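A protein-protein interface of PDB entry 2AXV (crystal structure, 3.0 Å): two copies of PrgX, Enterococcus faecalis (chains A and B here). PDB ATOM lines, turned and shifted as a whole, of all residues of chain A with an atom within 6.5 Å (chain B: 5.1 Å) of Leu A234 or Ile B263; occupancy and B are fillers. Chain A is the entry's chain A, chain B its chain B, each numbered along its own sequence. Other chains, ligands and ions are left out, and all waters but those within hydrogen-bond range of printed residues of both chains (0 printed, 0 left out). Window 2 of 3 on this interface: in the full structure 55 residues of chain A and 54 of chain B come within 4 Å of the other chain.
Printed residues of chain A that touch a printed residue of chain B: Asp A233, Leu A234, Asn A237, Asn A256, Asn A259 and Ile A263.
Of the 11 printed residues of chain B, 4 touch a printed residue of chain A.
Hydrophobic or aromatic side chains of chain B within 4 Å of the printed part of chain A: Ile B263, Ile B266 and Ile B267.
Tyr A232 touches none of the printed residues of chain B.
Of the printed residues of chain B, Asp A233 touches Ile B267.
Printed residues of chain B within 4 Å of Asn A256: Ile B266.
Printed residues of chain B within 4 Å of Asn A259: Asn B259 (3.0 Å) and Ile B263 (3.6 Å).
Of the printed residues of chain B, Ile A263 touches Asn B259 (3.8 Å) and Ile B263 (3.1 Å).
Of the printed residues of chain A, Ile B263 touches Leu A234, Asn A259 and Ile A263.
Of the printed residues of chain A, Ile B267 touches Asp A233 (3.7 Å) and Asn A237 (3.5 Å).
Gly B268 touches none of the printed residues of chain A.
The nearest printed residue of chain A that does not touch Ile B263 is Ile A260 (4.005 Å).
The side-chain amide oxygen (OD1) of Asn B259 lies within hydrogen-bond range of the side-chain amide nitrogen (ND2) of Asn A259 (3.0 Å).
OD2 of Asp A233 is in hydrogen-bond range of ND2 of Asn A237 (3.0 Å).
Leu A234 touches Ile B263, but with the chains exchanged Ile A263 does not touch Leu B234 (4.6 Å).
Asn A259 touches its own counterpart, Asn B259.
Asn A259 touches Ile B263, and with the chains exchanged Ile A263 touches Asn B259.
Ile B263 touches its own counterpart, Ile A263.
Positions printed for both chains: 234, 259, 260, 263, 264 and 267.
Asp A233 touches Ile B267 (OD1 to O, 3.7 Å).
CG2 of Ile B263 touches CD2 of Leu A234, at 3.8 Å.
Ile B266 touches Asn A237 (O to OD1, 3.5 Å).
Asn A237 touches Ile B267.
Ile B266 touches Asn A256 (CD1 to OD1, 3.9 Å).
CD1 of Ile B263 touches ND2 of Asn A259 (3.6 Å).
Asn B259 touches Ile A263 (ND2 to CD1, 3.8 Å).
Ile A263 touches Ile B263.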
ATOM      1  N   PHE A 217      15.876 -27.112 -31.675  1.00  0.00           N
ATOM      2  CA  PHE A 217      17.082 -27.445 -30.965  1.00  0.00           C
ATOM      3  C   PHE A 217      16.852 -28.692 -30.151  1.00  0.00           C
ATOM      4  O   PHE A 217      17.648 -29.616 -30.228  1.00  0.00           O
ATOM      5  CB  PHE A 217      17.501 -26.315 -30.056  1.00  0.00           C
ATOM      6  CG  PHE A 217      18.842 -26.523 -29.407  1.00  0.00           C
ATOM      7  CD1 PHE A 217      20.012 -26.353 -30.128  1.00  0.00           C
ATOM      8  CD2 PHE A 217      18.946 -26.857 -28.061  1.00  0.00           C
ATOM      9  CE1 PHE A 217      21.295 -26.546 -29.506  1.00  0.00           C
ATOM     10  CE2 PHE A 217      20.231 -27.037 -27.437  1.00  0.00           C
ATOM     11  CZ  PHE A 217      21.385 -26.885 -28.161  1.00  0.00           C
ATOM     12  N   ASN A 229      26.649 -28.935 -28.848  1.00  0.00           N
ATOM     13  CA  ASN A 229      27.535 -27.981 -28.230  1.00  0.00           C
ATOM     14  C   ASN A 229      26.982 -27.604 -26.857  1.00  0.00           C
ATOM     15  O   ASN A 229      25.899 -27.071 -26.766  1.00  0.00           O
ATOM     16  CB  ASN A 229      27.648 -26.769 -29.144  1.00  0.00           C
ATOM     17  CG  ASN A 229      28.648 -25.747 -28.652  1.00  0.00           C
ATOM     18  OD1 ASN A 229      28.854 -25.569 -27.450  1.00  0.00           O
ATOM     19  ND2 ASN A 229      29.246 -25.025 -29.592  1.00  0.00           N
ATOM     20  N   GLY A 230      27.714 -27.905 -25.797  1.00  0.00           N
ATOM     21  CA  GLY A 230      27.300 -27.569 -24.441  1.00  0.00           C
ATOM     22  C   GLY A 230      27.218 -26.092 -24.145  1.00  0.00           C
ATOM     23  O   GLY A 230      26.373 -25.679 -23.377  1.00  0.00           O
ATOM     24  N   TYR A 231      28.078 -25.269 -24.725  1.00  0.00           N
ATOM     25  CA  TYR A 231      27.971 -23.808 -24.507  1.00  0.00           C
ATOM     26  C   TYR A 231      26.668 -23.297 -25.143  1.00  0.00           C
ATOM     27  O   TYR A 231      25.958 -22.491 -24.576  1.00  0.00           O
ATOM     28  CB  TYR A 231      29.180 -23.037 -25.074  1.00  0.00           C
ATOM     29  CG  TYR A 231      30.569 -23.332 -24.492  1.00  0.00           C
ATOM     30  CD1 TYR A 231      30.904 -22.990 -23.221  1.00  0.00           C
ATOM     31  CD2 TYR A 231      31.556 -23.910 -25.268  1.00  0.00           C
ATOM     32  CE1 TYR A 231      32.182 -23.261 -22.732  1.00  0.00           C
ATOM     33  CE2 TYR A 231      32.795 -24.146 -24.811  1.00  0.00           C
ATOM     34  CZ  TYR A 231      33.120 -23.816 -23.556  1.00  0.00           C
ATOM     35  OH  TYR A 231      34.380 -24.089 -23.110  1.00  0.00           O
ATOM     36  N   TYR A 232      26.368 -23.798 -26.319  1.00  0.00           N
ATOM     37  CA  TYR A 232      25.093 -23.586 -26.917  1.00  0.00           C
ATOM     38  C   TYR A 232      23.936 -24.119 -26.047  1.00  0.00           C
ATOM     39  O   TYR A 232      22.937 -23.407 -25.880  1.00  0.00           O
ATOM     40  CB  TYR A 232      25.073 -24.267 -28.280  1.00  0.00           C
ATOM     41  CG  TYR A 232      25.839 -23.578 -29.409  1.00  0.00           C
ATOM     42  CD1 TYR A 232      25.768 -24.080 -30.722  1.00  0.00           C
ATOM     43  CD2 TYR A 232      26.589 -22.437 -29.204  1.00  0.00           C
ATOM     44  CE1 TYR A 232      26.420 -23.460 -31.794  1.00  0.00           C
ATOM     45  CE2 TYR A 232      27.263 -21.839 -30.249  1.00  0.00           C
ATOM     46  CZ  TYR A 232      27.177 -22.345 -31.534  1.00  0.00           C
ATOM     47  OH  TYR A 232      27.859 -21.711 -32.535  1.00  0.00           O
ATOM     48  N   ASP A 233      24.053 -25.340 -25.498  1.00  0.00           N
ATOM     49  CA  ASP A 233      22.952 -25.939 -24.697  1.00  0.00           C
ATOM     50  C   ASP A 233      22.675 -24.941 -23.575  1.00  0.00           C
ATOM     51  O   ASP A 233      21.544 -24.591 -23.302  1.00  0.00           O
ATOM     52  CB  ASP A 233      23.234 -27.413 -24.186  1.00  0.00           C
ATOM     53  CG  ASP A 233      21.923 -28.168 -23.633  1.00  0.00           C
ATOM     54  OD1 ASP A 233      21.940 -29.330 -23.081  1.00  0.00           O
ATOM     55  OD2 ASP A 233      20.837 -27.563 -23.708  1.00  0.00           O
ATOM     56  N   LEU A 234      23.732 -24.426 -22.983  1.00  0.00           N
ATOM     57  CA  LEU A 234      23.598 -23.489 -21.890  1.00  0.00           C
ATOM     58  C   LEU A 234      22.873 -22.230 -22.283  1.00  0.00           C
ATOM     59  O   LEU A 234      21.953 -21.793 -21.603  1.00  0.00           O
ATOM     60  CB  LEU A 234      24.976 -23.090 -21.372  1.00  0.00           C
ATOM     61  CG  LEU A 234      25.408 -23.754 -20.071  1.00  0.00           C
ATOM     62  CD1 LEU A 234      26.853 -23.347 -19.761  1.00  0.00           C
ATOM     63  CD2 LEU A 234      24.472 -23.373 -18.900  1.00  0.00           C
ATOM     64  N   GLU A 235      23.313 -21.643 -23.379  1.00  0.00           N
ATOM     65  CA  GLU A 235      22.868 -20.333 -23.779  1.00  0.00           C
ATOM     66  C   GLU A 235      21.434 -20.352 -24.313  1.00  0.00           C
ATOM     67  O   GLU A 235      20.628 -19.487 -24.044  1.00  0.00           O
ATOM     68  CB  GLU A 235      23.825 -19.884 -24.835  1.00  0.00           C
ATOM     69  CG  GLU A 235      23.801 -18.429 -25.138  1.00  0.00           C
ATOM     70  CD  GLU A 235      24.714 -18.151 -26.300  1.00  0.00           C
ATOM     71  OE1 GLU A 235      24.199 -17.584 -27.299  1.00  0.00           O
ATOM     72  OE2 GLU A 235      25.926 -18.567 -26.218  1.00  0.00           O
ATOM     73  N   ILE A 236      21.140 -21.366 -25.082  1.00  0.00           N
ATOM     74  CA  ILE A 236      19.812 -21.625 -25.507  1.00  0.00           C
ATOM     75  C   ILE A 236      18.972 -21.883 -24.290  1.00  0.00           C
ATOM     76  O   ILE A 236      17.819 -21.445 -24.259  1.00  0.00           O
ATOM     77  CB  ILE A 236      19.792 -22.787 -26.491  1.00  0.00           C
ATOM     78  CG1 ILE A 236      20.307 -22.251 -27.836  1.00  0.00           C
ATOM     79  CG2 ILE A 236      18.418 -23.410 -26.600  1.00  0.00           C
ATOM     80  CD1 ILE A 236      20.430 -23.252 -28.905  1.00  0.00           C
ATOM     81  N   ASN A 237      19.514 -22.564 -23.278  1.00  0.00           N
ATOM     82  CA  ASN A 237      18.726 -22.799 -22.058  1.00  0.00           C
ATOM     83  C   ASN A 237      18.415 -21.490 -21.318  1.00  0.00           C
ATOM     84  O   ASN A 237      17.326 -21.282 -20.782  1.00  0.00           O
ATOM     85  CB  ASN A 237      19.352 -23.876 -21.150  1.00  0.00           C
ATOM     86  CG  ASN A 237      18.487 -25.159 -21.101  1.00  0.00           C
ATOM     87  OD1 ASN A 237      17.481 -25.212 -20.353  1.00  0.00           O
ATOM     88  ND2 ASN A 237      18.865 -26.188 -21.884  1.00  0.00           N
ATOM     89  N   TYR A 238      19.373 -20.593 -21.339  1.00  0.00           N
ATOM     90  CA  TYR A 238      19.157 -19.276 -20.835  1.00  0.00           C
ATOM     91  C   TYR A 238      18.054 -18.556 -21.575  1.00  0.00           C
ATOM     92  O   TYR A 238      17.293 -17.854 -20.963  1.00  0.00           O
ATOM     93  CB  TYR A 238      20.457 -18.491 -20.933  1.00  0.00           C
ATOM     94  CG  TYR A 238      20.243 -17.043 -21.250  1.00  0.00           C
ATOM     95  CD1 TYR A 238      20.271 -16.597 -22.553  1.00  0.00           C
ATOM     96  CD2 TYR A 238      20.009 -16.116 -20.227  1.00  0.00           C
ATOM     97  CE1 TYR A 238      20.080 -15.271 -22.848  1.00  0.00           C
ATOM     98  CE2 TYR A 238      19.808 -14.784 -20.504  1.00  0.00           C
ATOM     99  CZ  TYR A 238      19.840 -14.368 -21.826  1.00  0.00           C
ATOM    100  OH  TYR A 238      19.648 -13.050 -22.138  1.00  0.00           O
ATOM    101  N   LEU A 239      17.988 -18.731 -22.886  1.00  0.00           N
ATOM    102  CA  LEU A 239      16.926 -18.156 -23.687  1.00  0.00           C
ATOM    103  C   LEU A 239      15.558 -18.791 -23.421  1.00  0.00           C
ATOM    104  O   LEU A 239      14.556 -18.115 -23.427  1.00  0.00           O
ATOM    105  CB  LEU A 239      17.224 -18.325 -25.151  1.00  0.00           C
ATOM    106  CG  LEU A 239      18.436 -17.573 -25.614  1.00  0.00           C
ATOM    107  CD1 LEU A 239      18.795 -18.008 -27.038  1.00  0.00           C
ATOM    108  CD2 LEU A 239      18.225 -16.068 -25.552  1.00  0.00           C
ATOM    109  N   ASN A 256      16.771 -17.934 -12.920  1.00  0.00           N
ATOM    110  CA  ASN A 256      17.497 -18.968 -13.635  1.00  0.00           C
ATOM    111  C   ASN A 256      18.319 -18.378 -14.758  1.00  0.00           C
ATOM    112  O   ASN A 256      19.488 -18.705 -14.940  1.00  0.00           O
ATOM    113  CB  ASN A 256      16.545 -19.940 -14.331  1.00  0.00           C
ATOM    114  CG  ASN A 256      15.869 -20.927 -13.423  1.00  0.00           C
ATOM    115  OD1 ASN A 256      16.281 -21.165 -12.307  1.00  0.00           O
ATOM    116  ND2 ASN A 256      14.819 -21.543 -13.936  1.00  0.00           N
ATOM    117  N   ASN A 259      21.194 -16.737 -13.343  1.00  0.00           N
ATOM    118  CA  ASN A 259      22.108 -17.706 -12.831  1.00  0.00           C
ATOM    119  C   ASN A 259      22.963 -18.267 -13.958  1.00  0.00           C
ATOM    120  O   ASN A 259      24.161 -18.397 -13.797  1.00  0.00           O
ATOM    121  CB  ASN A 259      21.362 -18.809 -12.086  1.00  0.00           C
ATOM    122  CG  ASN A 259      22.299 -19.741 -11.379  1.00  0.00           C
ATOM    123  OD1 ASN A 259      23.422 -19.373 -11.054  1.00  0.00           O
ATOM    124  ND2 ASN A 259      21.866 -20.961 -11.157  1.00  0.00           N
ATOM    125  N   ILE A 260      22.365 -18.543 -15.109  1.00  0.00           N
ATOM    126  CA  ILE A 260      23.114 -19.084 -16.235  1.00  0.00           C
ATOM    127  C   ILE A 260      24.124 -18.054 -16.744  1.00  0.00           C
ATOM    128  O   ILE A 260      25.275 -18.403 -17.063  1.00  0.00           O
ATOM    129  CB  ILE A 260      22.205 -19.523 -17.372  1.00  0.00           C
ATOM    130  CG1 ILE A 260      21.300 -20.646 -16.893  1.00  0.00           C
ATOM    131  CG2 ILE A 260      23.055 -19.989 -18.595  1.00  0.00           C
ATOM    132  CD1 ILE A 260      20.290 -21.069 -17.903  1.00  0.00           C
ATOM    133  N   ILE A 263      27.052 -18.169 -14.686  1.00  0.00           N
ATOM    134  CA  ILE A 263      27.858 -19.357 -14.801  1.00  0.00           C
ATOM    135  C   ILE A 263      28.854 -19.234 -15.965  1.00  0.00           C
ATOM    136  O   ILE A 263      29.976 -19.674 -15.856  1.00  0.00           O
ATOM    137  CB  ILE A 263      26.981 -20.586 -14.783  1.00  0.00           C
ATOM    138  CG1 ILE A 263      27.444 -21.451 -13.627  1.00  0.00           C
ATOM    139  CG2 ILE A 263      27.038 -21.347 -16.040  1.00  0.00           C
ATOM    140  CD1 ILE A 263      26.397 -22.346 -13.136  1.00  0.00           C
ATOM    141  N   PHE A 264      28.447 -18.595 -17.057  1.00  0.00           N
ATOM    142  CA  PHE A 264      29.395 -18.286 -18.121  1.00  0.00           C
ATOM    143  C   PHE A 264      30.575 -17.481 -17.559  1.00  0.00           C
ATOM    144  O   PHE A 264      31.754 -17.805 -17.841  1.00  0.00           O
ATOM    145  CB  PHE A 264      28.759 -17.529 -19.283  1.00  0.00           C
ATOM    146  CG  PHE A 264      28.020 -18.414 -20.237  1.00  0.00           C
ATOM    147  CD1 PHE A 264      28.705 -19.189 -21.146  1.00  0.00           C
ATOM    148  CD2 PHE A 264      26.636 -18.483 -20.215  1.00  0.00           C
ATOM    149  CE1 PHE A 264      28.031 -20.027 -22.032  1.00  0.00           C
ATOM    150  CE2 PHE A 264      25.957 -19.315 -21.094  1.00  0.00           C
ATOM    151  CZ  PHE A 264      26.668 -20.093 -22.011  1.00  0.00           C
ATOM    152  N   ILE A 267      32.972 -19.666 -15.561  1.00  0.00           N
ATOM    153  CA  ILE A 267      33.838 -20.612 -16.275  1.00  0.00           C
ATOM    154  C   ILE A 267      34.651 -19.887 -17.331  1.00  0.00           C
ATOM    155  O   ILE A 267      35.230 -20.515 -18.223  1.00  0.00           O
ATOM    156  CB  ILE A 267      33.090 -21.781 -16.895  1.00  0.00           C
ATOM    157  CG1 ILE A 267      32.258 -21.307 -18.082  1.00  0.00           C
ATOM    158  CG2 ILE A 267      32.246 -22.482 -15.838  1.00  0.00           C
ATOM    159  CD1 ILE A 267      31.689 -22.413 -18.863  1.00  0.00           C
ATOM    160  N   LEU A 276      25.214 -11.791 -23.053  1.00  0.00           N
ATOM    161  CA  LEU A 276      24.011 -12.171 -22.346  1.00  0.00           C
ATOM    162  C   LEU A 276      23.617 -11.133 -21.308  1.00  0.00           C
ATOM    163  O   LEU A 276      22.430 -10.865 -21.080  1.00  0.00           O
ATOM    164  CB  LEU A 276      24.188 -13.530 -21.707  1.00  0.00           C
ATOM    165  CG  LEU A 276      24.528 -14.682 -22.654  1.00  0.00           C
ATOM    166  CD1 LEU A 276      23.947 -15.949 -22.105  1.00  0.00           C
ATOM    167  CD2 LEU A 276      24.078 -14.492 -24.096  1.00  0.00           C
ATOM    168  N   LEU B 234      32.066 -27.184 -17.974  1.00  0.00           N
ATOM    169  CA  LEU B 234      31.271 -27.005 -16.771  1.00  0.00           C
ATOM    170  C   LEU B 234      31.655 -27.945 -15.715  1.00  0.00           C
ATOM    171  O   LEU B 234      31.851 -27.520 -14.598  1.00  0.00           O
ATOM    172  CB  LEU B 234      29.805 -27.266 -16.971  1.00  0.00           C
ATOM    173  CG  LEU B 234      29.050 -25.976 -16.758  1.00  0.00           C
ATOM    174  CD1 LEU B 234      27.588 -26.302 -16.848  1.00  0.00           C
ATOM    175  CD2 LEU B 234      29.374 -25.287 -15.423  1.00  0.00           C
ATOM    176  N   ASN B 259      25.951 -25.127  -7.170  1.00  0.00           N
ATOM    177  CA  ASN B 259      25.292 -24.377  -8.167  1.00  0.00           C
ATOM    178  C   ASN B 259      25.406 -25.001  -9.546  1.00  0.00           C
ATOM    179  O   ASN B 259      24.435 -25.094 -10.297  1.00  0.00           O
ATOM    180  CB  ASN B 259      25.887 -23.014  -8.183  1.00  0.00           C
ATOM    181  CG  ASN B 259      25.159 -22.116  -9.120  1.00  0.00           C
ATOM    182  OD1 ASN B 259      23.967 -22.332  -9.459  1.00  0.00           O
ATOM    183  ND2 ASN B 259      25.853 -21.084  -9.570  1.00  0.00           N
ATOM    184  N   ILE B 260      26.614 -25.449  -9.856  1.00  0.00           N
ATOM    185  CA  ILE B 260      26.895 -26.059 -11.120  1.00  0.00           C
ATOM    186  C   ILE B 260      26.099 -27.347 -11.270  1.00  0.00           C
ATOM    187  O   ILE B 260      25.526 -27.618 -12.345  1.00  0.00           O
ATOM    188  CB  ILE B 260      28.357 -26.344 -11.230  1.00  0.00           C
ATOM    189  CG1 ILE B 260      29.104 -25.021 -11.350  1.00  0.00           C
ATOM    190  CG2 ILE B 260      28.602 -27.267 -12.460  1.00  0.00           C
ATOM    191  CD1 ILE B 260      30.606 -25.135 -11.353  1.00  0.00           C
ATOM    192  N   ILE B 261      26.074 -28.132 -10.187  1.00  0.00           N
ATOM    193  CA  ILE B 261      25.290 -29.393 -10.145  1.00  0.00           C
ATOM    194  C   ILE B 261      23.903 -29.105 -10.575  1.00  0.00           C
ATOM    195  O   ILE B 261      23.281 -29.836 -11.333  1.00  0.00           O
ATOM    196  CB  ILE B 261      25.167 -30.050  -8.711  1.00  0.00           C
ATOM    197  CG1 ILE B 261      26.489 -30.710  -8.297  1.00  0.00           C
ATOM    198  CG2 ILE B 261      24.162 -31.152  -8.734  1.00  0.00           C
ATOM    199  CD1 ILE B 261      26.657 -31.043  -6.840  1.00  0.00           C
ATOM    200  N   ASN B 262      23.419 -28.011 -10.048  1.00  0.00           N
ATOM    201  CA  ASN B 262      22.086 -27.607 -10.281  1.00  0.00           C
ATOM    202  C   ASN B 262      21.808 -27.162 -11.692  1.00  0.00           C
ATOM    203  O   ASN B 262      20.751 -27.402 -12.242  1.00  0.00           O
ATOM    204  CB  ASN B 262      21.793 -26.465  -9.341  1.00  0.00           C
ATOM    205  CG  ASN B 262      20.363 -26.284  -9.187  1.00  0.00           C
ATOM    206  OD1 ASN B 262      19.801 -25.365  -9.784  1.00  0.00           O
ATOM    207  ND2 ASN B 262      19.700 -27.236  -8.484  1.00  0.00           N
ATOM    208  N   ILE B 263      22.785 -26.513 -12.282  1.00  0.00           N
ATOM    209  CA  ILE B 263      22.660 -26.042 -13.656  1.00  0.00           C
ATOM    210  C   ILE B 263      22.512 -27.191 -14.638  1.00  0.00           C
ATOM    211  O   ILE B 263      21.671 -27.156 -15.512  1.00  0.00           O
ATOM    212  CB  ILE B 263      23.878 -25.153 -13.980  1.00  0.00           C
ATOM    213  CG1 ILE B 263      23.709 -23.854 -13.216  1.00  0.00           C
ATOM    214  CG2 ILE B 263      24.073 -24.946 -15.483  1.00  0.00           C
ATOM    215  CD1 ILE B 263      23.148 -22.717 -14.006  1.00  0.00           C
ATOM    216  N   PHE B 264      23.319 -28.224 -14.483  1.00  0.00           N
ATOM    217  CA  PHE B 264      23.118 -29.388 -15.288  1.00  0.00           C
ATOM    218  C   PHE B 264      21.655 -29.802 -15.176  1.00  0.00           C
ATOM    219  O   PHE B 264      21.013 -30.029 -16.203  1.00  0.00           O
ATOM    220  CB  PHE B 264      24.071 -30.499 -14.874  1.00  0.00           C
ATOM    221  CG  PHE B 264      25.494 -30.313 -15.366  1.00  0.00           C
ATOM    222  CD1 PHE B 264      25.810 -30.520 -16.685  1.00  0.00           C
ATOM    223  CD2 PHE B 264      26.518 -29.997 -14.498  1.00  0.00           C
ATOM    224  CE1 PHE B 264      27.097 -30.369 -17.135  1.00  0.00           C
ATOM    225  CE2 PHE B 264      27.794 -29.857 -14.961  1.00  0.00           C
ATOM    226  CZ  PHE B 264      28.071 -30.042 -16.279  1.00  0.00           C
ATOM    227  N   LYS B 265      21.130 -29.871 -13.952  1.00  0.00           N
ATOM    228  CA  LYS B 265      19.727 -30.232 -13.735  1.00  0.00           C
ATOM    229  C   LYS B 265      18.830 -29.372 -14.561  1.00  0.00           C
ATOM    230  O   LYS B 265      18.012 -29.866 -15.317  1.00  0.00           O
ATOM    231  CB  LYS B 265      19.359 -30.035 -12.253  1.00  0.00           C
ATOM    232  CG  LYS B 265      17.843 -29.980 -11.913  1.00  0.00           C
ATOM    233  CD  LYS B 265      17.563 -29.368 -10.489  1.00  0.00           C
ATOM    234  CE  LYS B 265      16.966 -27.946 -10.543  1.00  0.00           C
ATOM    235  NZ  LYS B 265      16.778 -27.294  -9.200  1.00  0.00           N
ATOM    236  N   ILE B 266      19.005 -28.082 -14.400  1.00  0.00           N
ATOM    237  CA  ILE B 266      18.263 -27.101 -15.148  1.00  0.00           C
ATOM    238  C   ILE B 266      18.259 -27.288 -16.646  1.00  0.00           C
ATOM    239  O   ILE B 266      17.269 -26.983 -17.299  1.00  0.00           O
ATOM    240  CB  ILE B 266      18.844 -25.689 -14.925  1.00  0.00           C
ATOM    241  CG1 ILE B 266      18.367 -25.125 -13.615  1.00  0.00           C
ATOM    242  CG2 ILE B 266      18.432 -24.690 -15.986  1.00  0.00           C
ATOM    243  CD1 ILE B 266      19.036 -23.840 -13.222  1.00  0.00           C
ATOM    244  N   ILE B 267      19.370 -27.736 -17.216  1.00  0.00           N
ATOM    245  CA  ILE B 267      19.487 -27.801 -18.666  1.00  0.00           C
ATOM    246  C   ILE B 267      19.240 -29.222 -19.159  1.00  0.00           C
ATOM    247  O   ILE B 267      19.431 -29.534 -20.346  1.00  0.00           O
ATOM    248  CB  ILE B 267      20.841 -27.208 -19.166  1.00  0.00           C
ATOM    249  CG1 ILE B 267      22.023 -28.034 -18.709  1.00  0.00           C
ATOM    250  CG2 ILE B 267      21.043 -25.775 -18.662  1.00  0.00           C
ATOM    251  CD1 ILE B 267      23.178 -27.850 -19.593  1.00  0.00           C
ATOM    252  N   GLY B 268      18.809 -30.075 -18.239  1.00  0.00           N
ATOM    253  CA  GLY B 268      18.272 -31.348 -18.618  1.00  0.00           C
ATOM    254  C   GLY B 268      19.285 -32.448 -18.720  1.00  0.00           C
ATOM    255  O   GLY B 268      18.963 -33.511 -19.234  1.00  0.00           O
